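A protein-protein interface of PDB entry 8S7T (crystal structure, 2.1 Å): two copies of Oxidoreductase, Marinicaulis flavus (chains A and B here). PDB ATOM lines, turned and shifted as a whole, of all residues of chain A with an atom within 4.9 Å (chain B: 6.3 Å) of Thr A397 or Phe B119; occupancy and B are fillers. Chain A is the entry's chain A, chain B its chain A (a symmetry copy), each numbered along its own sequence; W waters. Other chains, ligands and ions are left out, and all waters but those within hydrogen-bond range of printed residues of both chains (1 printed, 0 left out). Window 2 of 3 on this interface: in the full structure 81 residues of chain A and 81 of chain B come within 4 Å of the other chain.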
ATOM      1  N   THR A 257      -3.129  17.565  17.781  1.00  0.00           N
ATOM      2  CA  THR A 257      -1.726  17.216  17.640  1.00  0.00           C
ATOM      3  C   THR A 257      -1.048  18.071  16.573  1.00  0.00           C
ATOM      4  O   THR A 257       0.073  18.510  16.809  1.00  0.00           O
ATOM      5  CB  THR A 257      -1.544  15.731  17.361  1.00  0.00           C
ATOM      6  OG1 THR A 257      -2.222  15.083  18.431  1.00  0.00           O
ATOM      7  CG2 THR A 257      -0.083  15.334  17.319  1.00  0.00           C
ATOM      8  N   GLU A 258      -1.713  18.303  15.429  1.00  0.00           N
ATOM      9  CA  GLU A 258      -1.179  19.186  14.391  1.00  0.00           C
ATOM     10  C   GLU A 258      -0.886  20.584  14.955  1.00  0.00           C
ATOM     11  O   GLU A 258       0.117  21.200  14.610  1.00  0.00           O
ATOM     12  CB  GLU A 258      -2.168  19.337  13.228  1.00  0.00           C
ATOM     13  CG  GLU A 258      -2.217  18.135  12.317  1.00  0.00           C
ATOM     14  CD  GLU A 258      -0.879  17.841  11.679  1.00  0.00           C
ATOM     15  OE1 GLU A 258      -0.425  18.696  10.877  1.00  0.00           O
ATOM     16  OE2 GLU A 258      -0.264  16.803  12.041  1.00  0.00           O
ATOM     17  N   ARG A 261       2.131  20.865  17.464  1.00  0.00           N
ATOM     18  CA  ARG A 261       3.466  20.622  16.922  1.00  0.00           C
ATOM     19  C   ARG A 261       4.297  21.902  16.912  1.00  0.00           C
ATOM     20  O   ARG A 261       5.347  21.935  17.547  1.00  0.00           O
ATOM     21  CB  ARG A 261       3.440  20.013  15.514  1.00  0.00           C
ATOM     22  CG  ARG A 261       4.809  19.951  14.837  1.00  0.00           C
ATOM     23  CD  ARG A 261       4.838  19.200  13.517  1.00  0.00           C
ATOM     24  NE  ARG A 261       3.897  19.785  12.575  1.00  0.00           N
ATOM     25  CZ  ARG A 261       2.766  19.218  12.157  1.00  0.00           C
ATOM     26  NH1 ARG A 261       2.368  18.029  12.596  1.00  0.00           N
ATOM     27  NH2 ARG A 261       2.014  19.870  11.298  1.00  0.00           N
ATOM     28  N   VAL A 265       7.716  22.632  19.274  1.00  0.00           N
ATOM     29  CA  VAL A 265       9.025  22.724  18.641  1.00  0.00           C
ATOM     30  C   VAL A 265       9.660  24.080  18.978  1.00  0.00           C
ATOM     31  O   VAL A 265      10.837  24.158  19.321  1.00  0.00           O
ATOM     32  CB  VAL A 265       8.916  22.475  17.122  1.00  0.00           C
ATOM     33  CG1 VAL A 265      10.244  22.693  16.416  1.00  0.00           C
ATOM     34  CG2 VAL A 265       8.399  21.087  16.800  1.00  0.00           C
ATOM     35  N   PRO A 395       6.363  10.604  15.531  1.00  0.00           N
ATOM     36  CA  PRO A 395       6.349  12.011  15.117  1.00  0.00           C
ATOM     37  C   PRO A 395       5.149  12.786  15.662  1.00  0.00           C
ATOM     38  O   PRO A 395       4.058  12.235  15.791  1.00  0.00           O
ATOM     39  CB  PRO A 395       6.286  11.949  13.568  1.00  0.00           C
ATOM     40  CG  PRO A 395       6.829  10.561  13.227  1.00  0.00           C
ATOM     41  CD  PRO A 395       6.419   9.668  14.387  1.00  0.00           C
ATOM     42  N   ILE A 396       5.323  14.092  15.937  1.00  0.00           N
ATOM     43  CA  ILE A 396       4.199  14.904  16.374  1.00  0.00           C
ATOM     44  C   ILE A 396       3.350  15.212  15.150  1.00  0.00           C
ATOM     45  O   ILE A 396       3.469  16.280  14.554  1.00  0.00           O
ATOM     46  CB  ILE A 396       4.601  16.194  17.113  1.00  0.00           C
ATOM     47  CG1 ILE A 396       5.627  15.936  18.217  1.00  0.00           C
ATOM     48  CG2 ILE A 396       3.363  16.929  17.660  1.00  0.00           C
ATOM     49  CD1 ILE A 396       6.304  17.199  18.693  1.00  0.00           C
ATOM     50  N   THR A 397       2.450  14.278  14.846  1.00  0.00           N
ATOM     51  CA  THR A 397       1.564  14.389  13.696  1.00  0.00           C
ATOM     52  C   THR A 397       0.158  13.962  14.104  1.00  0.00           C
ATOM     53  O   THR A 397      -0.019  13.016  14.853  1.00  0.00           O
ATOM     54  CB  THR A 397       2.229  13.590  12.565  1.00  0.00           C
ATOM     55  OG1 THR A 397       3.021  14.501  11.794  1.00  0.00           O
ATOM     56  CG2 THR A 397       1.290  12.845  11.675  1.00  0.00           C
ATOM     57  N   GLY A 398      -0.848  14.687  13.615  1.00  0.00           N
ATOM     58  CA  GLY A 398      -2.230  14.286  13.767  1.00  0.00           C
ATOM     59  C   GLY A 398      -2.467  12.846  13.343  1.00  0.00           C
ATOM     60  O   GLY A 398      -3.126  12.096  14.061  1.00  0.00           O
ATOM     61  N   LYS A 399      -1.926  12.481  12.175  1.00  0.00           N
ATOM     62  CA  LYS A 399      -2.115  11.158  11.603  1.00  0.00           C
ATOM     63  C   LYS A 399      -1.546  10.109  12.541  1.00  0.00           C
ATOM     64  O   LYS A 399      -2.128   9.056  12.717  1.00  0.00           O
ATOM     65  CB  LYS A 399      -1.477  11.060  10.209  1.00  0.00           C
ATOM     66  CG  LYS A 399      -2.193  11.842   9.109  1.00  0.00           C
ATOM     67  CD  LYS A 399      -3.641  11.387   8.898  1.00  0.00           C
ATOM     68  CE  LYS A 399      -4.333  11.982   7.692  1.00  0.00           C
ATOM     69  NZ  LYS A 399      -5.746  11.538   7.639  1.00  0.00           N
ATOM     70  N   ASP A 400      -0.382  10.377  13.113  1.00  0.00           N
ATOM     71  CA  ASP A 400       0.256   9.383  13.955  1.00  0.00           C
ATOM     72  C   ASP A 400      -0.558   9.294  15.245  1.00  0.00           C
ATOM     73  O   ASP A 400      -0.753   8.220  15.768  1.00  0.00           O
ATOM     74  CB  ASP A 400       1.720   9.729  14.242  1.00  0.00           C
ATOM     75  CG  ASP A 400       2.667   9.481  13.074  1.00  0.00           C
ATOM     76  OD1 ASP A 400       2.893   8.300  12.762  1.00  0.00           O
ATOM     77  OD2 ASP A 400       3.197  10.467  12.510  1.00  0.00           O
ATOM     78  N   ALA A 401      -1.006  10.445  15.749  1.00  0.00           N
ATOM     79  CA  ALA A 401      -1.736  10.504  17.003  1.00  0.00           C
ATOM     80  C   ALA A 401      -3.009   9.666  16.885  1.00  0.00           C
ATOM     81  O   ALA A 401      -3.234   8.792  17.724  1.00  0.00           O
ATOM     82  CB  ALA A 401      -2.026  11.944  17.364  1.00  0.00           C
ATOM     83  N   ARG A 428      10.255  17.531  20.598  1.00  0.00           N
ATOM     84  CA  ARG A 428       9.947  17.187  19.215  1.00  0.00           C
ATOM     85  C   ARG A 428       9.350  15.782  19.141  1.00  0.00           C
ATOM     86  O   ARG A 428       9.135  15.255  18.047  1.00  0.00           O
ATOM     87  CB  ARG A 428      11.238  17.263  18.392  1.00  0.00           C
ATOM     88  CG  ARG A 428      11.712  18.673  18.081  1.00  0.00           C
ATOM     89  CD  ARG A 428      13.084  18.614  17.458  1.00  0.00           C
ATOM     90  NE  ARG A 428      13.466  19.913  16.936  1.00  0.00           N
ATOM     91  CZ  ARG A 428      13.890  20.938  17.657  1.00  0.00           C
ATOM     92  NH1 ARG A 428      14.043  20.839  18.961  1.00  0.00           N
ATOM     93  NH2 ARG A 428      14.206  22.067  17.051  1.00  0.00           N
ATOM     94  N   LEU A 430       6.499  12.869  20.171  1.00  0.00           N
ATOM     95  CA  LEU A 430       5.176  12.469  20.598  1.00  0.00           C
ATOM     96  C   LEU A 430       5.249  11.063  21.192  1.00  0.00           C
ATOM     97  O   LEU A 430       5.854  10.174  20.603  1.00  0.00           O
ATOM     98  CB  LEU A 430       4.241  12.479  19.384  1.00  0.00           C
ATOM     99  CG  LEU A 430       2.807  12.037  19.686  1.00  0.00           C
ATOM    100  CD1 LEU A 430       2.076  13.115  20.498  1.00  0.00           C
ATOM    101  CD2 LEU A 430       2.045  11.761  18.411  1.00  0.00           C
ATOM    102  N   ASN B 116      14.116  19.227   7.882  1.00  0.00           N
ATOM    103  CA  ASN B 116      12.708  19.111   8.170  1.00  0.00           C
ATOM    104  C   ASN B 116      12.242  20.389   8.846  1.00  0.00           C
ATOM    105  O   ASN B 116      12.645  20.698   9.962  1.00  0.00           O
ATOM    106  CB  ASN B 116      12.466  17.899   9.051  1.00  0.00           C
ATOM    107  CG  ASN B 116      11.004  17.556   9.124  1.00  0.00           C
ATOM    108  OD1 ASN B 116      10.193  18.387   9.501  1.00  0.00           O
ATOM    109  ND2 ASN B 116      10.690  16.328   8.773  1.00  0.00           N
ATOM    110  N   GLU B 117      11.397  21.139   8.169  1.00  0.00           N
ATOM    111  CA  GLU B 117      11.005  22.425   8.701  1.00  0.00           C
ATOM    112  C   GLU B 117      10.038  22.227   9.867  1.00  0.00           C
ATOM    113  O   GLU B 117      10.182  22.885  10.885  1.00  0.00           O
ATOM    114  CB  GLU B 117      10.357  23.262   7.606  1.00  0.00           C
ATOM    115  CG  GLU B 117       9.868  24.600   8.100  1.00  0.00           C
ATOM    116  CD  GLU B 117       9.384  25.467   6.958  1.00  0.00           C
ATOM    117  OE1 GLU B 117       8.642  24.925   6.158  1.00  0.00           O
ATOM    118  OE2 GLU B 117       9.773  26.662   6.865  1.00  0.00           O
ATOM    119  N   GLU B 118       9.082  21.304   9.702  1.00  0.00           N
ATOM    120  CA  GLU B 118       7.958  21.132  10.609  1.00  0.00           C
ATOM    121  C   GLU B 118       8.463  20.642  11.970  1.00  0.00           C
ATOM    122  O   GLU B 118       7.915  21.009  12.995  1.00  0.00           O
ATOM    123  CB  GLU B 118       6.961  20.127  10.013  1.00  0.00           C
ATOM    124  CG  GLU B 118       6.270  20.604   8.736  1.00  0.00           C
ATOM    125  CD  GLU B 118       7.102  20.735   7.457  1.00  0.00           C
ATOM    126  OE1 GLU B 118       8.158  20.079   7.339  1.00  0.00           O
ATOM    127  OE2 GLU B 118       6.701  21.530   6.571  1.00  0.00           O
ATOM    128  N   PHE B 119       9.511  19.806  11.969  1.00  0.00           N
ATOM    129  CA  PHE B 119      10.099  19.270  13.185  1.00  0.00           C
ATOM    130  C   PHE B 119      11.407  19.963  13.586  1.00  0.00           C
ATOM    131  O   PHE B 119      11.979  19.645  14.638  1.00  0.00           O
ATOM    132  CB  PHE B 119      10.308  17.771  13.000  1.00  0.00           C
ATOM    133  CG  PHE B 119       8.996  17.048  12.874  1.00  0.00           C
ATOM    134  CD1 PHE B 119       8.048  17.148  13.881  1.00  0.00           C
ATOM    135  CD2 PHE B 119       8.690  16.311  11.743  1.00  0.00           C
ATOM    136  CE1 PHE B 119       6.837  16.485  13.772  1.00  0.00           C
ATOM    137  CE2 PHE B 119       7.469  15.661  11.634  1.00  0.00           C
ATOM    138  CZ  PHE B 119       6.549  15.757  12.645  1.00  0.00           C
ATOM    139  N   GLY B 120      11.885  20.901  12.759  1.00  0.00           N
ATOM    140  CA  GLY B 120      13.067  21.689  13.096  1.00  0.00           C
ATOM    141  C   GLY B 120      14.310  20.825  13.279  1.00  0.00           C
ATOM    142  O   GLY B 120      14.858  20.757  14.370  1.00  0.00           O
ATOM    143  N   TYR B 121      14.745  20.147  12.210  1.00  0.00           N
ATOM    144  CA  TYR B 121      15.993  19.415  12.258  1.00  0.00           C
ATOM    145  C   TYR B 121      16.634  19.271  10.878  1.00  0.00           C
ATOM    146  O   TYR B 121      16.020  19.518   9.852  1.00  0.00           O
ATOM    147  CB  TYR B 121      15.774  18.040  12.896  1.00  0.00           C
ATOM    148  CG  TYR B 121      15.024  17.007  12.095  1.00  0.00           C
ATOM    149  CD1 TYR B 121      15.634  16.346  11.046  1.00  0.00           C
ATOM    150  CD2 TYR B 121      13.739  16.612  12.445  1.00  0.00           C
ATOM    151  CE1 TYR B 121      14.970  15.369  10.326  1.00  0.00           C
ATOM    152  CE2 TYR B 121      13.066  15.613  11.758  1.00  0.00           C
ATOM    153  CZ  TYR B 121      13.680  15.004  10.669  1.00  0.00           C
ATOM    154  OH  TYR B 121      13.089  14.015   9.921  1.00  0.00           O
ATOM    155  N   LEU B 144      13.990  28.379   9.432  1.00  0.00           N
ATOM    156  CA  LEU B 144      14.845  27.729  10.398  1.00  0.00           C
ATOM    157  C   LEU B 144      16.134  28.533  10.483  1.00  0.00           C
ATOM    158  O   LEU B 144      16.629  29.005   9.456  1.00  0.00           O
ATOM    159  CB  LEU B 144      15.159  26.312   9.903  1.00  0.00           C
ATOM    160  CG  LEU B 144      14.017  25.296   9.842  1.00  0.00           C
ATOM    161  CD1 LEU B 144      14.563  23.970   9.345  1.00  0.00           C
ATOM    162  CD2 LEU B 144      13.356  25.112  11.216  1.00  0.00           C
ATOM    163  N   ASN B 201      10.491   7.044  11.992  1.00  0.00           N
ATOM    164  CA  ASN B 201      10.570   8.388  11.480  1.00  0.00           C
ATOM    165  C   ASN B 201      10.957   9.318  12.623  1.00  0.00           C
ATOM    166  O   ASN B 201      10.545  10.466  12.634  1.00  0.00           O
ATOM    167  CB  ASN B 201       9.235   8.812  10.858  1.00  0.00           C
ATOM    168  CG  ASN B 201       8.910   8.022   9.604  1.00  0.00           C
ATOM    169  OD1 ASN B 201       7.986   7.216   9.586  1.00  0.00           O
ATOM    170  ND2 ASN B 201       9.699   8.197   8.561  1.00  0.00           N
ATOM    171  N   GLN B 204      15.552  11.841  14.434  1.00  0.00           N
ATOM    172  CA  GLN B 204      15.917  13.205  14.792  1.00  0.00           C
ATOM    173  C   GLN B 204      14.894  13.840  15.745  1.00  0.00           C
ATOM    174  O   GLN B 204      14.862  15.067  15.877  1.00  0.00           O
ATOM    175  CB  GLN B 204      16.082  14.052  13.522  1.00  0.00           C
ATOM    176  CG  GLN B 204      17.458  13.923  12.886  1.00  0.00           C
ATOM    177  CD  GLN B 204      17.792  12.506  12.472  1.00  0.00           C
ATOM    178  OE1 GLN B 204      17.267  11.999  11.492  1.00  0.00           O
ATOM    179  NE2 GLN B 204      18.692  11.855  13.195  1.00  0.00           N
ATOM    180  N   LEU B 205      14.061  13.035  16.424  1.00  0.00           N
ATOM    181  CA  LEU B 205      13.006  13.606  17.263  1.00  0.00           C
ATOM    182  C   LEU B 205      13.186  13.243  18.731  1.00  0.00           C
ATOM    183  O   LEU B 205      12.606  13.884  19.614  1.00  0.00           O
ATOM    184  CB  LEU B 205      11.639  13.125  16.774  1.00  0.00           C
ATOM    185  CG  LEU B 205      11.283  13.471  15.334  1.00  0.00           C
ATOM    186  CD1 LEU B 205       9.863  13.046  15.057  1.00  0.00           C
ATOM    187  CD2 LEU B 205      11.462  14.946  15.033  1.00  0.00           C
ATOM    188  N   TRP B 232      19.216  19.463  15.888  1.00  0.00           N
ATOM    189  CA  TRP B 232      17.996  20.210  15.998  1.00  0.00           C
ATOM    190  C   TRP B 232      18.279  21.618  15.532  1.00  0.00           C
ATOM    191  O   TRP B 232      19.346  22.155  15.835  1.00  0.00           O
ATOM    192  CB  TRP B 232      17.460  20.181  17.433  1.00  0.00           C
ATOM    193  CG  TRP B 232      16.962  18.834  17.868  1.00  0.00           C
ATOM    194  CD1 TRP B 232      16.527  17.810  17.082  1.00  0.00           C
ATOM    195  CD2 TRP B 232      16.905  18.347  19.217  1.00  0.00           C
ATOM    196  NE1 TRP B 232      16.184  16.732  17.846  1.00  0.00           N
ATOM    197  CE2 TRP B 232      16.421  17.029  19.159  1.00  0.00           C
ATOM    198  CE3 TRP B 232      17.202  18.907  20.461  1.00  0.00           C
ATOM    199  CZ2 TRP B 232      16.178  16.270  20.303  1.00  0.00           C
ATOM    200  CZ3 TRP B 232      16.991  18.146  21.593  1.00  0.00           C
ATOM    201  CH2 TRP B 232      16.499  16.837  21.508  1.00  0.00           C
ATOM    202  N   LEU B 233      17.267  22.213  14.885  1.00  0.00           N
ATOM    203  CA  LEU B 233      17.334  23.561  14.333  1.00  0.00           C
ATOM    204  C   LEU B 233      16.233  24.436  14.907  1.00  0.00           C
ATOM    205  O   LEU B 233      15.083  24.030  14.897  1.00  0.00           O
ATOM    206  CB  LEU B 233      17.133  23.440  12.822  1.00  0.00           C
ATOM    207  CG  LEU B 233      18.224  22.686  12.082  1.00  0.00           C
ATOM    208  CD1 LEU B 233      18.009  22.841  10.585  1.00  0.00           C
ATOM    209  CD2 LEU B 233      19.605  23.204  12.501  1.00  0.00           C
HETATM  210  O   HOH W   1      12.552  15.878  21.381  1.00  0.00           O
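The guanidinium group (NE) of Arg A428 is in hydrogen-bond range of the backbone carbonyl oxygen (O) of Phe B119 (2.8 Å).
O of Gly B120 sits at hydrogen-bond distance from NE of Arg A428 (3.0 Å).
The backbone carbonyl oxygen (O) of Leu B233 lies within hydrogen-bond range of the guanidinium group (NH2) of Arg A428, 3.0 Å away.
The side-chain carboxylate of Glu A258 is in salt-bridge range of the guanidinium group of Arg A261, at 2.7 Å.
NH1 of Arg A261 is in hydrogen-bond range of O of Ile A396 (2.8 Å).
OD1 of Asn B116 lies within hydrogen-bond range of N of Glu B118.
The side-chain amide oxygen (OD1) of Asn B116 sits at hydrogen-bond distance from the backbone NH (N) of Phe B119 (2.9 Å).
The backbone NH of Leu B233 sits at hydrogen-bond distance from the backbone carbonyl oxygen of Gly B120 (2.9 Å).
The backbone carbonyl oxygen of Gln B204 is in hydrogen-bond range of the indole nitrogen of Trp B232 (2.9 Å).
Among the printed residues, merely in contact across the chains: Arg A261 with Glu B118 (3.6 Å), Arg A261 with Phe B119 (3.4 Å), Val A265 with Glu B118 (3.8 Å), Val A265 with Phe B119 (3.9 Å), Pro A395 with Phe B119 (3.9 Å), Pro A395 with Asn B201 (3.8 Å), Pro A395 with Leu B205 (3.7 Å), Ile A396 with Phe B119 (3.5 Å), Thr A397 with Phe B119 (3.8 Å), Arg A428 with Leu B205 (3.5 Å) and Arg A428 with Trp B232 (3.6 Å).
Printed residues of chain B within 4 Å of Arg A261: Glu B118 (3.6 Å) and Phe B119 (3.4 Å).
Of chain B, only Phe B119 (3.8 Å) comes within 4 Å of Thr A397.
Leu A430 touches none of the printed residues of chain B.
Glu B117 touches none of the printed residues of chain A.
Of the printed residues of chain A, Phe B119 touches Arg A261, Val A265, Pro A395, Ile A396, Thr A397 and Arg A428.
Printed residues of chain A within 4 Å of Trp B232: Arg A428 (3.6 Å).
The nearest printed residue of chain B that does not touch Thr A397 is Glu B118 (7.1 Å).
The nearest printed residue of chain A that does not touch Phe B119 is Asp A400 (6.3 Å).
Among the printed residues, 14 pairs touch across the chains.
Among the printed residues, no Asp or Glu carboxylate lies within 4 Å of a Lys or Arg side-chain nitrogen of the other chain.
No position is printed for both chains.
Water W1 lies within hydrogen-bond range of the backbone carbonyl oxygen of Leu B205 (2.7 Å) and the backbone NH of Arg A428 (2.9 Å).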
